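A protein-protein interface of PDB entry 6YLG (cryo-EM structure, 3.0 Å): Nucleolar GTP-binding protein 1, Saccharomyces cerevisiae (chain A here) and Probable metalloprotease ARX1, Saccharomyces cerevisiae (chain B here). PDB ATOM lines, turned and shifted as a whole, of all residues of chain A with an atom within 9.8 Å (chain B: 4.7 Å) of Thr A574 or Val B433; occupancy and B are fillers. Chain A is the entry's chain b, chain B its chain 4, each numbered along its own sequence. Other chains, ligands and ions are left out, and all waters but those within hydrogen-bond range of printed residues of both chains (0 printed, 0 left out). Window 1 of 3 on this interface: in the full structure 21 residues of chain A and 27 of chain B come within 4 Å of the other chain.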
ATOM      1  N   PHE A 567     -19.780 -23.198 -18.896  1.00  0.00           N
ATOM      2  CA  PHE A 567     -20.419 -24.345 -19.535  1.00  0.00           C
ATOM      3  C   PHE A 567     -19.690 -25.665 -19.295  1.00  0.00           C
ATOM      4  O   PHE A 567     -19.838 -26.603 -20.084  1.00  0.00           O
ATOM      5  CB  PHE A 567     -20.532 -24.087 -21.040  1.00  0.00           C
ATOM      6  CG  PHE A 567     -21.471 -22.974 -21.405  1.00  0.00           C
ATOM      7  CD1 PHE A 567     -22.823 -23.058 -21.121  1.00  0.00           C
ATOM      8  CD2 PHE A 567     -20.998 -21.840 -22.037  1.00  0.00           C
ATOM      9  CE1 PHE A 567     -23.676 -22.031 -21.463  1.00  0.00           C
ATOM     10  CE2 PHE A 567     -21.847 -20.816 -22.381  1.00  0.00           C
ATOM     11  CZ  PHE A 567     -23.186 -20.911 -22.092  1.00  0.00           C
ATOM     12  N   ASP A 571     -24.948 -28.402 -19.412  1.00  0.00           N
ATOM     13  CA  ASP A 571     -25.132 -29.076 -20.687  1.00  0.00           C
ATOM     14  C   ASP A 571     -26.599 -28.973 -21.075  1.00  0.00           C
ATOM     15  O   ASP A 571     -27.394 -28.311 -20.405  1.00  0.00           O
ATOM     16  CB  ASP A 571     -24.694 -30.545 -20.621  1.00  0.00           C
ATOM     17  CG  ASP A 571     -25.617 -31.389 -19.766  1.00  0.00           C
ATOM     18  OD1 ASP A 571     -26.167 -30.859 -18.779  1.00  0.00           O
ATOM     19  OD2 ASP A 571     -25.791 -32.586 -20.082  1.00  0.00           O
ATOM     20  N   ALA A 572     -26.940 -29.627 -22.183  1.00  0.00           N
ATOM     21  CA  ALA A 572     -28.327 -29.802 -22.598  1.00  0.00           C
ATOM     22  C   ALA A 572     -29.000 -28.477 -22.932  1.00  0.00           C
ATOM     23  O   ALA A 572     -30.188 -28.291 -22.647  1.00  0.00           O
ATOM     24  CB  ALA A 572     -29.125 -30.535 -21.515  1.00  0.00           C
ATOM     25  N   LEU A 573     -28.253 -27.552 -23.530  1.00  0.00           N
ATOM     26  CA  LEU A 573     -28.861 -26.442 -24.247  1.00  0.00           C
ATOM     27  C   LEU A 573     -29.293 -26.944 -25.618  1.00  0.00           C
ATOM     28  O   LEU A 573     -28.519 -27.616 -26.305  1.00  0.00           O
ATOM     29  CB  LEU A 573     -27.880 -25.279 -24.388  1.00  0.00           C
ATOM     30  CG  LEU A 573     -28.437 -23.858 -24.278  1.00  0.00           C
ATOM     31  CD1 LEU A 573     -27.303 -22.851 -24.261  1.00  0.00           C
ATOM     32  CD2 LEU A 573     -29.397 -23.557 -25.422  1.00  0.00           C
ATOM     33  N   THR A 574     -30.522 -26.613 -26.019  1.00  0.00           N
ATOM     34  CA  THR A 574     -31.199 -27.211 -27.166  1.00  0.00           C
ATOM     35  C   THR A 574     -31.160 -28.726 -27.032  1.00  0.00           C
ATOM     36  O   THR A 574     -30.511 -29.410 -27.834  1.00  0.00           O
ATOM     37  CB  THR A 574     -30.567 -26.772 -28.489  1.00  0.00           C
ATOM     38  OG1 THR A 574     -29.282 -27.389 -28.639  1.00  0.00           O
ATOM     39  CG2 THR A 574     -30.416 -25.262 -28.536  1.00  0.00           C
ATOM     40  N   ALA A 575     -31.955 -29.183 -26.064  1.00  0.00           N
ATOM     41  CA  ALA A 575     -31.962 -30.582 -25.660  1.00  0.00           C
ATOM     42  C   ALA A 575     -32.299 -31.506 -26.830  1.00  0.00           C
ATOM     43  O   ALA A 575     -32.770 -31.082 -27.890  1.00  0.00           O
ATOM     44  CB  ALA A 575     -32.962 -30.808 -24.527  1.00  0.00           C
ATOM     45  N   SER A 576     -32.044 -32.795 -26.613  1.00  0.00           N
ATOM     46  CA  SER A 576     -32.230 -33.975 -27.451  1.00  0.00           C
ATOM     47  C   SER A 576     -33.539 -33.885 -28.223  1.00  0.00           C
ATOM     48  O   SER A 576     -34.621 -33.841 -27.628  1.00  0.00           O
ATOM     49  CB  SER A 576     -32.208 -35.231 -26.587  1.00  0.00           C
ATOM     50  OG  SER A 576     -30.892 -35.740 -26.466  1.00  0.00           O
ATOM     51  N   THR A 577     -33.685 -33.568 -29.505  1.00  0.00           N
ATOM     52  CA  THR A 577     -34.920 -33.857 -30.214  1.00  0.00           C
ATOM     53  C   THR A 577     -35.107 -35.369 -30.342  1.00  0.00           C
ATOM     54  O   THR A 577     -34.214 -36.164 -30.037  1.00  0.00           O
ATOM     55  CB  THR A 577     -34.916 -33.197 -31.596  1.00  0.00           C
ATOM     56  OG1 THR A 577     -36.187 -33.388 -32.229  1.00  0.00           O
ATOM     57  CG2 THR A 577     -33.823 -33.776 -32.485  1.00  0.00           C
ATOM     58  N   GLU A 578     -36.293 -35.763 -30.808  1.00  0.00           N
ATOM     59  CA  GLU A 578     -36.635 -37.181 -30.826  1.00  0.00           C
ATOM     60  C   GLU A 578     -35.900 -37.923 -31.936  1.00  0.00           C
ATOM     61  O   GLU A 578     -35.156 -38.873 -31.665  1.00  0.00           O
ATOM     62  CB  GLU A 578     -38.144 -37.354 -30.980  1.00  0.00           C
ATOM     63  CG  GLU A 578     -38.939 -36.957 -29.744  1.00  0.00           C
ATOM     64  CD  GLU A 578     -39.316 -35.488 -29.740  1.00  0.00           C
ATOM     65  OE1 GLU A 578     -40.522 -35.183 -29.836  1.00  0.00           O
ATOM     66  OE2 GLU A 578     -38.406 -34.640 -29.639  1.00  0.00           O
ATOM     67  N   GLY A 580     -33.470 -37.139 -33.803  1.00  0.00           N
ATOM     68  CA  GLY A 580     -32.085 -36.784 -34.040  1.00  0.00           C
ATOM     69  C   GLY A 580     -31.905 -35.954 -35.291  1.00  0.00           C
ATOM     70  O   GLY A 580     -31.040 -36.241 -36.123  1.00  0.00           O
ATOM     71  N   VAL A 581     -32.729 -34.917 -35.424  1.00  0.00           N
ATOM     72  CA  VAL A 581     -32.758 -34.061 -36.598  1.00  0.00           C
ATOM     73  C   VAL A 581     -32.185 -32.699 -36.235  1.00  0.00           C
ATOM     74  O   VAL A 581     -32.082 -32.329 -35.065  1.00  0.00           O
ATOM     75  CB  VAL A 581     -34.178 -33.904 -37.177  1.00  0.00           C
ATOM     76  CG1 VAL A 581     -34.745 -35.253 -37.575  1.00  0.00           C
ATOM     77  CG2 VAL A 581     -35.103 -33.166 -36.208  1.00  0.00           C
ATOM     78  N   LYS A 582     -31.809 -31.958 -37.269  1.00  0.00           N
ATOM     79  CA  LYS A 582     -31.252 -30.627 -37.125  1.00  0.00           C
ATOM     80  C   LYS A 582     -32.382 -29.601 -37.057  1.00  0.00           C
ATOM     81  O   LYS A 582     -33.562 -29.941 -36.944  1.00  0.00           O
ATOM     82  CB  LYS A 582     -30.288 -30.340 -38.275  1.00  0.00           C
ATOM     83  CG  LYS A 582     -29.179 -31.370 -38.418  1.00  0.00           C
ATOM     84  CD  LYS A 582     -28.231 -31.011 -39.542  1.00  0.00           C
ATOM     85  CE  LYS A 582     -27.139 -32.054 -39.703  1.00  0.00           C
ATOM     86  NZ  LYS A 582     -26.402 -31.886 -40.986  1.00  0.00           N
ATOM     87  N   LEU A 583     -32.015 -28.322 -37.120  1.00  0.00           N
ATOM     88  CA  LEU A 583     -32.999 -27.261 -36.948  1.00  0.00           C
ATOM     89  C   LEU A 583     -33.936 -27.178 -38.147  1.00  0.00           C
ATOM     90  O   LEU A 583     -35.120 -26.852 -38.001  1.00  0.00           O
ATOM     91  CB  LEU A 583     -32.277 -25.933 -36.723  1.00  0.00           C
ATOM     92  CG  LEU A 583     -33.127 -24.696 -36.450  1.00  0.00           C
ATOM     93  CD1 LEU A 583     -32.793 -24.136 -35.082  1.00  0.00           C
ATOM     94  CD2 LEU A 583     -32.910 -23.640 -37.520  1.00  0.00           C
ATOM     95  N   ARG A 584     -33.422 -27.469 -39.341  1.00  0.00           N
ATOM     96  CA  ARG A 584     -34.189 -27.430 -40.580  1.00  0.00           C
ATOM     97  C   ARG A 584     -34.081 -28.789 -41.267  1.00  0.00           C
ATOM     98  O   ARG A 584     -33.189 -28.992 -42.098  1.00  0.00           O
ATOM     99  CB  ARG A 584     -33.667 -26.326 -41.505  1.00  0.00           C
ATOM    100  CG  ARG A 584     -33.380 -24.979 -40.855  1.00  0.00           C
ATOM    101  CD  ARG A 584     -32.707 -24.064 -41.869  1.00  0.00           C
ATOM    102  NE  ARG A 584     -32.479 -22.711 -41.369  1.00  0.00           N
ATOM    103  CZ  ARG A 584     -31.565 -22.377 -40.460  1.00  0.00           C
ATOM    104  NH1 ARG A 584     -30.764 -23.289 -39.920  1.00  0.00           N
ATOM    105  NH2 ARG A 584     -31.447 -21.113 -40.086  1.00  0.00           N
ATOM    106  N   ILE B 258     -31.622 -18.167 -21.500  1.00  0.00           N
ATOM    107  CA  ILE B 258     -31.088 -19.286 -22.266  1.00  0.00           C
ATOM    108  C   ILE B 258     -30.271 -20.181 -21.345  1.00  0.00           C
ATOM    109  O   ILE B 258     -30.578 -21.366 -21.177  1.00  0.00           O
ATOM    110  CB  ILE B 258     -30.237 -18.779 -23.445  1.00  0.00           C
ATOM    111  CG1 ILE B 258     -31.108 -18.000 -24.440  1.00  0.00           C
ATOM    112  CG2 ILE B 258     -29.505 -19.933 -24.112  1.00  0.00           C
ATOM    113  CD1 ILE B 258     -30.602 -16.608 -24.720  1.00  0.00           C
ATOM    114  N   ALA B 359     -28.166 -10.555 -32.454  1.00  0.00           N
ATOM    115  CA  ALA B 359     -27.307 -11.105 -31.417  1.00  0.00           C
ATOM    116  C   ALA B 359     -27.443 -12.620 -31.361  1.00  0.00           C
ATOM    117  O   ALA B 359     -28.530 -13.163 -31.582  1.00  0.00           O
ATOM    118  CB  ALA B 359     -27.653 -10.494 -30.062  1.00  0.00           C
ATOM    119  N   TYR B 360     -26.334 -13.295 -31.069  1.00  0.00           N
ATOM    120  CA  TYR B 360     -26.297 -14.734 -30.864  1.00  0.00           C
ATOM    121  C   TYR B 360     -25.566 -15.030 -29.563  1.00  0.00           C
ATOM    122  O   TYR B 360     -25.103 -14.116 -28.881  1.00  0.00           O
ATOM    123  CB  TYR B 360     -25.603 -15.446 -32.028  1.00  0.00           C
ATOM    124  CG  TYR B 360     -26.288 -15.272 -33.364  1.00  0.00           C
ATOM    125  CD1 TYR B 360     -27.263 -16.163 -33.786  1.00  0.00           C
ATOM    126  CD2 TYR B 360     -25.955 -14.223 -34.208  1.00  0.00           C
ATOM    127  CE1 TYR B 360     -27.887 -16.014 -35.005  1.00  0.00           C
ATOM    128  CE2 TYR B 360     -26.574 -14.065 -35.426  1.00  0.00           C
ATOM    129  CZ  TYR B 360     -27.541 -14.963 -35.820  1.00  0.00           C
ATOM    130  OH  TYR B 360     -28.163 -14.813 -37.037  1.00  0.00           O
ATOM    131  N   VAL B 361     -25.478 -16.313 -29.215  1.00  0.00           N
ATOM    132  CA  VAL B 361     -24.750 -16.763 -28.031  1.00  0.00           C
ATOM    133  C   VAL B 361     -24.502 -18.257 -28.183  1.00  0.00           C
ATOM    134  O   VAL B 361     -25.393 -18.987 -28.631  1.00  0.00           O
ATOM    135  CB  VAL B 361     -25.518 -16.458 -26.731  1.00  0.00           C
ATOM    136  CG1 VAL B 361     -26.812 -17.259 -26.653  1.00  0.00           C
ATOM    137  CG2 VAL B 361     -24.645 -16.715 -25.516  1.00  0.00           C
ATOM    138  N   GLN B 366     -21.538 -27.770 -26.326  1.00  0.00           N
ATOM    139  CA  GLN B 366     -21.726 -28.635 -27.485  1.00  0.00           C
ATOM    140  C   GLN B 366     -20.624 -28.423 -28.515  1.00  0.00           C
ATOM    141  O   GLN B 366     -19.977 -27.372 -28.562  1.00  0.00           O
ATOM    142  CB  GLN B 366     -23.084 -28.381 -28.135  1.00  0.00           C
ATOM    143  CG  GLN B 366     -23.486 -29.453 -29.143  1.00  0.00           C
ATOM    144  CD  GLN B 366     -24.635 -29.027 -30.031  1.00  0.00           C
ATOM    145  OE1 GLN B 366     -25.421 -28.159 -29.666  1.00  0.00           O
ATOM    146  NE2 GLN B 366     -24.733 -29.634 -31.207  1.00  0.00           N
ATOM    147  N   TYR B 430     -26.858 -27.163 -33.470  1.00  0.00           N
ATOM    148  CA  TYR B 430     -27.297 -26.377 -32.316  1.00  0.00           C
ATOM    149  C   TYR B 430     -26.121 -25.792 -31.541  1.00  0.00           C
ATOM    150  O   TYR B 430     -26.056 -25.897 -30.317  1.00  0.00           O
ATOM    151  CB  TYR B 430     -28.163 -27.237 -31.412  1.00  0.00           C
ATOM    152  CG  TYR B 430     -29.304 -27.918 -32.132  1.00  0.00           C
ATOM    153  CD1 TYR B 430     -30.503 -27.261 -32.352  1.00  0.00           C
ATOM    154  CD2 TYR B 430     -29.176 -29.218 -32.595  1.00  0.00           C
ATOM    155  CE1 TYR B 430     -31.543 -27.880 -33.007  1.00  0.00           C
ATOM    156  CE2 TYR B 430     -30.212 -29.843 -33.253  1.00  0.00           C
ATOM    157  CZ  TYR B 430     -31.393 -29.170 -33.457  1.00  0.00           C
ATOM    158  OH  TYR B 430     -32.428 -29.793 -34.111  1.00  0.00           O
ATOM    159  N   LEU B 431     -25.204 -25.118 -32.238  1.00  0.00           N
ATOM    160  CA  LEU B 431     -24.030 -24.533 -31.603  1.00  0.00           C
ATOM    161  C   LEU B 431     -24.299 -23.123 -31.096  1.00  0.00           C
ATOM    162  O   LEU B 431     -23.975 -22.810 -29.948  1.00  0.00           O
ATOM    163  CB  LEU B 431     -22.855 -24.509 -32.581  1.00  0.00           C
ATOM    164  CG  LEU B 431     -22.390 -25.852 -33.145  1.00  0.00           C
ATOM    165  CD1 LEU B 431     -21.282 -25.634 -34.151  1.00  0.00           C
ATOM    166  CD2 LEU B 431     -21.931 -26.788 -32.042  1.00  0.00           C
ATOM    167  N   CYS B 432     -24.880 -22.271 -31.935  1.00  0.00           N
ATOM    168  CA  CYS B 432     -25.285 -20.922 -31.573  1.00  0.00           C
ATOM    169  C   CYS B 432     -26.794 -20.794 -31.697  1.00  0.00           C
ATOM    170  O   CYS B 432     -27.443 -21.504 -32.470  1.00  0.00           O
ATOM    171  CB  CYS B 432     -24.613 -19.868 -32.457  1.00  0.00           C
ATOM    172  SG  CYS B 432     -22.832 -20.034 -32.618  1.00  0.00           S
ATOM    173  N   VAL B 433     -27.349 -19.878 -30.907  1.00  0.00           N
ATOM    174  CA  VAL B 433     -28.781 -19.627 -30.866  1.00  0.00           C
ATOM    175  C   VAL B 433     -28.999 -18.124 -30.884  1.00  0.00           C
ATOM    176  O   VAL B 433     -28.078 -17.343 -30.630  1.00  0.00           O
ATOM    177  CB  VAL B 433     -29.437 -20.259 -29.620  1.00  0.00           C
ATOM    178  CG1 VAL B 433     -29.038 -21.718 -29.498  1.00  0.00           C
ATOM    179  CG2 VAL B 433     -29.045 -19.494 -28.362  1.00  0.00           C
ATOM    180  N   GLU B 434     -30.231 -17.724 -31.184  1.00  0.00           N
ATOM    181  CA  GLU B 434     -30.571 -16.311 -31.233  1.00  0.00           C
ATOM    182  C   GLU B 434     -31.073 -15.834 -29.876  1.00  0.00           C
ATOM    183  O   GLU B 434     -31.803 -16.538 -29.174  1.00  0.00           O
ATOM    184  CB  GLU B 434     -31.643 -16.061 -32.291  1.00  0.00           C
ATOM    185  CG  GLU B 434     -31.239 -16.434 -33.706  1.00  0.00           C
ATOM    186  CD  GLU B 434     -32.406 -16.387 -34.675  1.00  0.00           C
ATOM    187  OE1 GLU B 434     -32.311 -15.666 -35.691  1.00  0.00           O
ATOM    188  OE2 GLU B 434     -33.420 -17.069 -34.420  1.00  0.00           O
ATOM    189  N   SER B 435     -30.673 -14.618 -29.507  1.00  0.00           N
ATOM    190  CA  SER B 435     -31.250 -13.933 -28.361  1.00  0.00           C
ATOM    191  C   SER B 435     -32.544 -13.276 -28.823  1.00  0.00           C
ATOM    192  O   SER B 435     -32.481 -12.346 -29.639  1.00  0.00           O
ATOM    193  CB  SER B 435     -30.289 -12.890 -27.798  1.00  0.00           C
ATOM    194  OG  SER B 435     -30.356 -11.685 -28.538  1.00  0.00           O
ATOM    195  N   THR B 465     -36.783 -24.336 -29.680  1.00  0.00           N
ATOM    196  CA  THR B 465     -35.408 -24.792 -29.882  1.00  0.00           C
ATOM    197  C   THR B 465     -34.546 -24.686 -28.631  1.00  0.00           C
ATOM    198  O   THR B 465     -33.554 -25.416 -28.513  1.00  0.00           O
ATOM    199  CB  THR B 465     -34.740 -24.030 -31.037  1.00  0.00           C
ATOM    200  OG1 THR B 465     -33.343 -24.349 -31.073  1.00  0.00           O
ATOM    201  CG2 THR B 465     -34.887 -22.511 -30.895  1.00  0.00           C
ATOM    202  N   LEU B 466     -34.891 -23.810 -27.686  1.00  0.00           N
ATOM    203  CA  LEU B 466     -34.024 -23.538 -26.537  1.00  0.00           C
ATOM    204  C   LEU B 466     -34.382 -24.346 -25.303  1.00  0.00           C
ATOM    205  O   LEU B 466     -33.508 -24.598 -24.460  1.00  0.00           O
ATOM    206  CB  LEU B 466     -34.070 -22.047 -26.209  1.00  0.00           C
ATOM    207  CG  LEU B 466     -33.421 -21.165 -27.278  1.00  0.00           C
ATOM    208  CD1 LEU B 466     -33.823 -19.716 -27.104  1.00  0.00           C
ATOM    209  CD2 LEU B 466     -31.904 -21.307 -27.279  1.00  0.00           C
ATOM    210  N   THR B 467     -35.647 -24.747 -25.171  1.00  0.00           N
ATOM    211  CA  THR B 467     -35.896 -25.676 -24.067  1.00  0.00           C
ATOM    212  C   THR B 467     -36.303 -25.013 -22.755  1.00  0.00           C
ATOM    213  O   THR B 467     -37.007 -25.643 -21.956  1.00  0.00           O
ATOM    214  CB  THR B 467     -34.652 -26.528 -23.789  1.00  0.00           C
ATOM    215  OG1 THR B 467     -33.659 -25.731 -23.126  1.00  0.00           O
ATOM    216  CG2 THR B 467     -34.061 -27.115 -25.082  1.00  0.00           C
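O of Val A581 is in hydrogen-bond range of OH of Tyr B430.
OH of Tyr B430 lies close to O of Lys A582 (3.1 Å).
The backbone NH (N) of Leu A583 lies within hydrogen-bond range of the side-chain hydroxyl (OH) of Tyr B430 (3.4 Å).
Leu A573 touches Ile B258.
Leu A573 touches Leu B466 (CD2 to CD2, 3.8 Å).
Tyr B430 touches Thr A574 (CB to OG1, 3.0 Å).
CG2 of Thr A574 touches CG1 of Val B433, 3.9 Å away.
Thr A574 touches Thr B465 (CG2 to O, 3.1 Å).
N of Thr A574 touches O of Leu B466, at 3.9 Å.
CG2 of Thr B467 touches CA of Thr A574, 3.5 Å away.
CG2 of Thr B467 touches N of Ala A575 (3.1 Å).
Of the printed residues of chain B, Leu A573 touches Ile B258 and Leu B466.
Of chain B, only Tyr B430, Val B433, Thr B465, Leu B466 and Thr B467 come within 4 Å of Thr A574.
Printed residues of chain B within 4 Å of Val A581: Tyr B430.
No residue of chain A comes within 4 Å of Cys B432.
Val B433 touches just one residue of chain A: Thr A574 (3.9 Å).
Leu B466 touches two residues of chain A.
Of the printed residues of chain A, Thr B467 touches Thr A574 and Ala A575.
The nearest residue of chain B that does not touch Thr A574 is Gln B366 (4.1 Å).
The nearest residue of chain A that does not touch Val B433 is Leu A573 (4.5 Å).
The nearest printed residue of chain B that does not touch Ala A575 is Thr B465 (4.8 Å).
The backbone carbonyl oxygen (O) of Val B361 is in hydrogen-bond range of the backbone NH (N) of Val B433 (3.1 Å).
OE1 of Gln B366 lies close to O of Tyr B430 (2.4 Å).
Of the 14 printed residues of chain A, 6 touch a printed residue of chain B.
Hydrophobic or aromatic side chains of chain A that line the printed part of chain B: Leu A573 and Ala A575.
Of the 14 printed residues of chain B, 6 touch a printed residue of chain A.
Hydrophobic or aromatic side chains of chain B within 4 Å of the printed part of chain A: Ile B258, Tyr B430, Val B433 and Leu B466.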
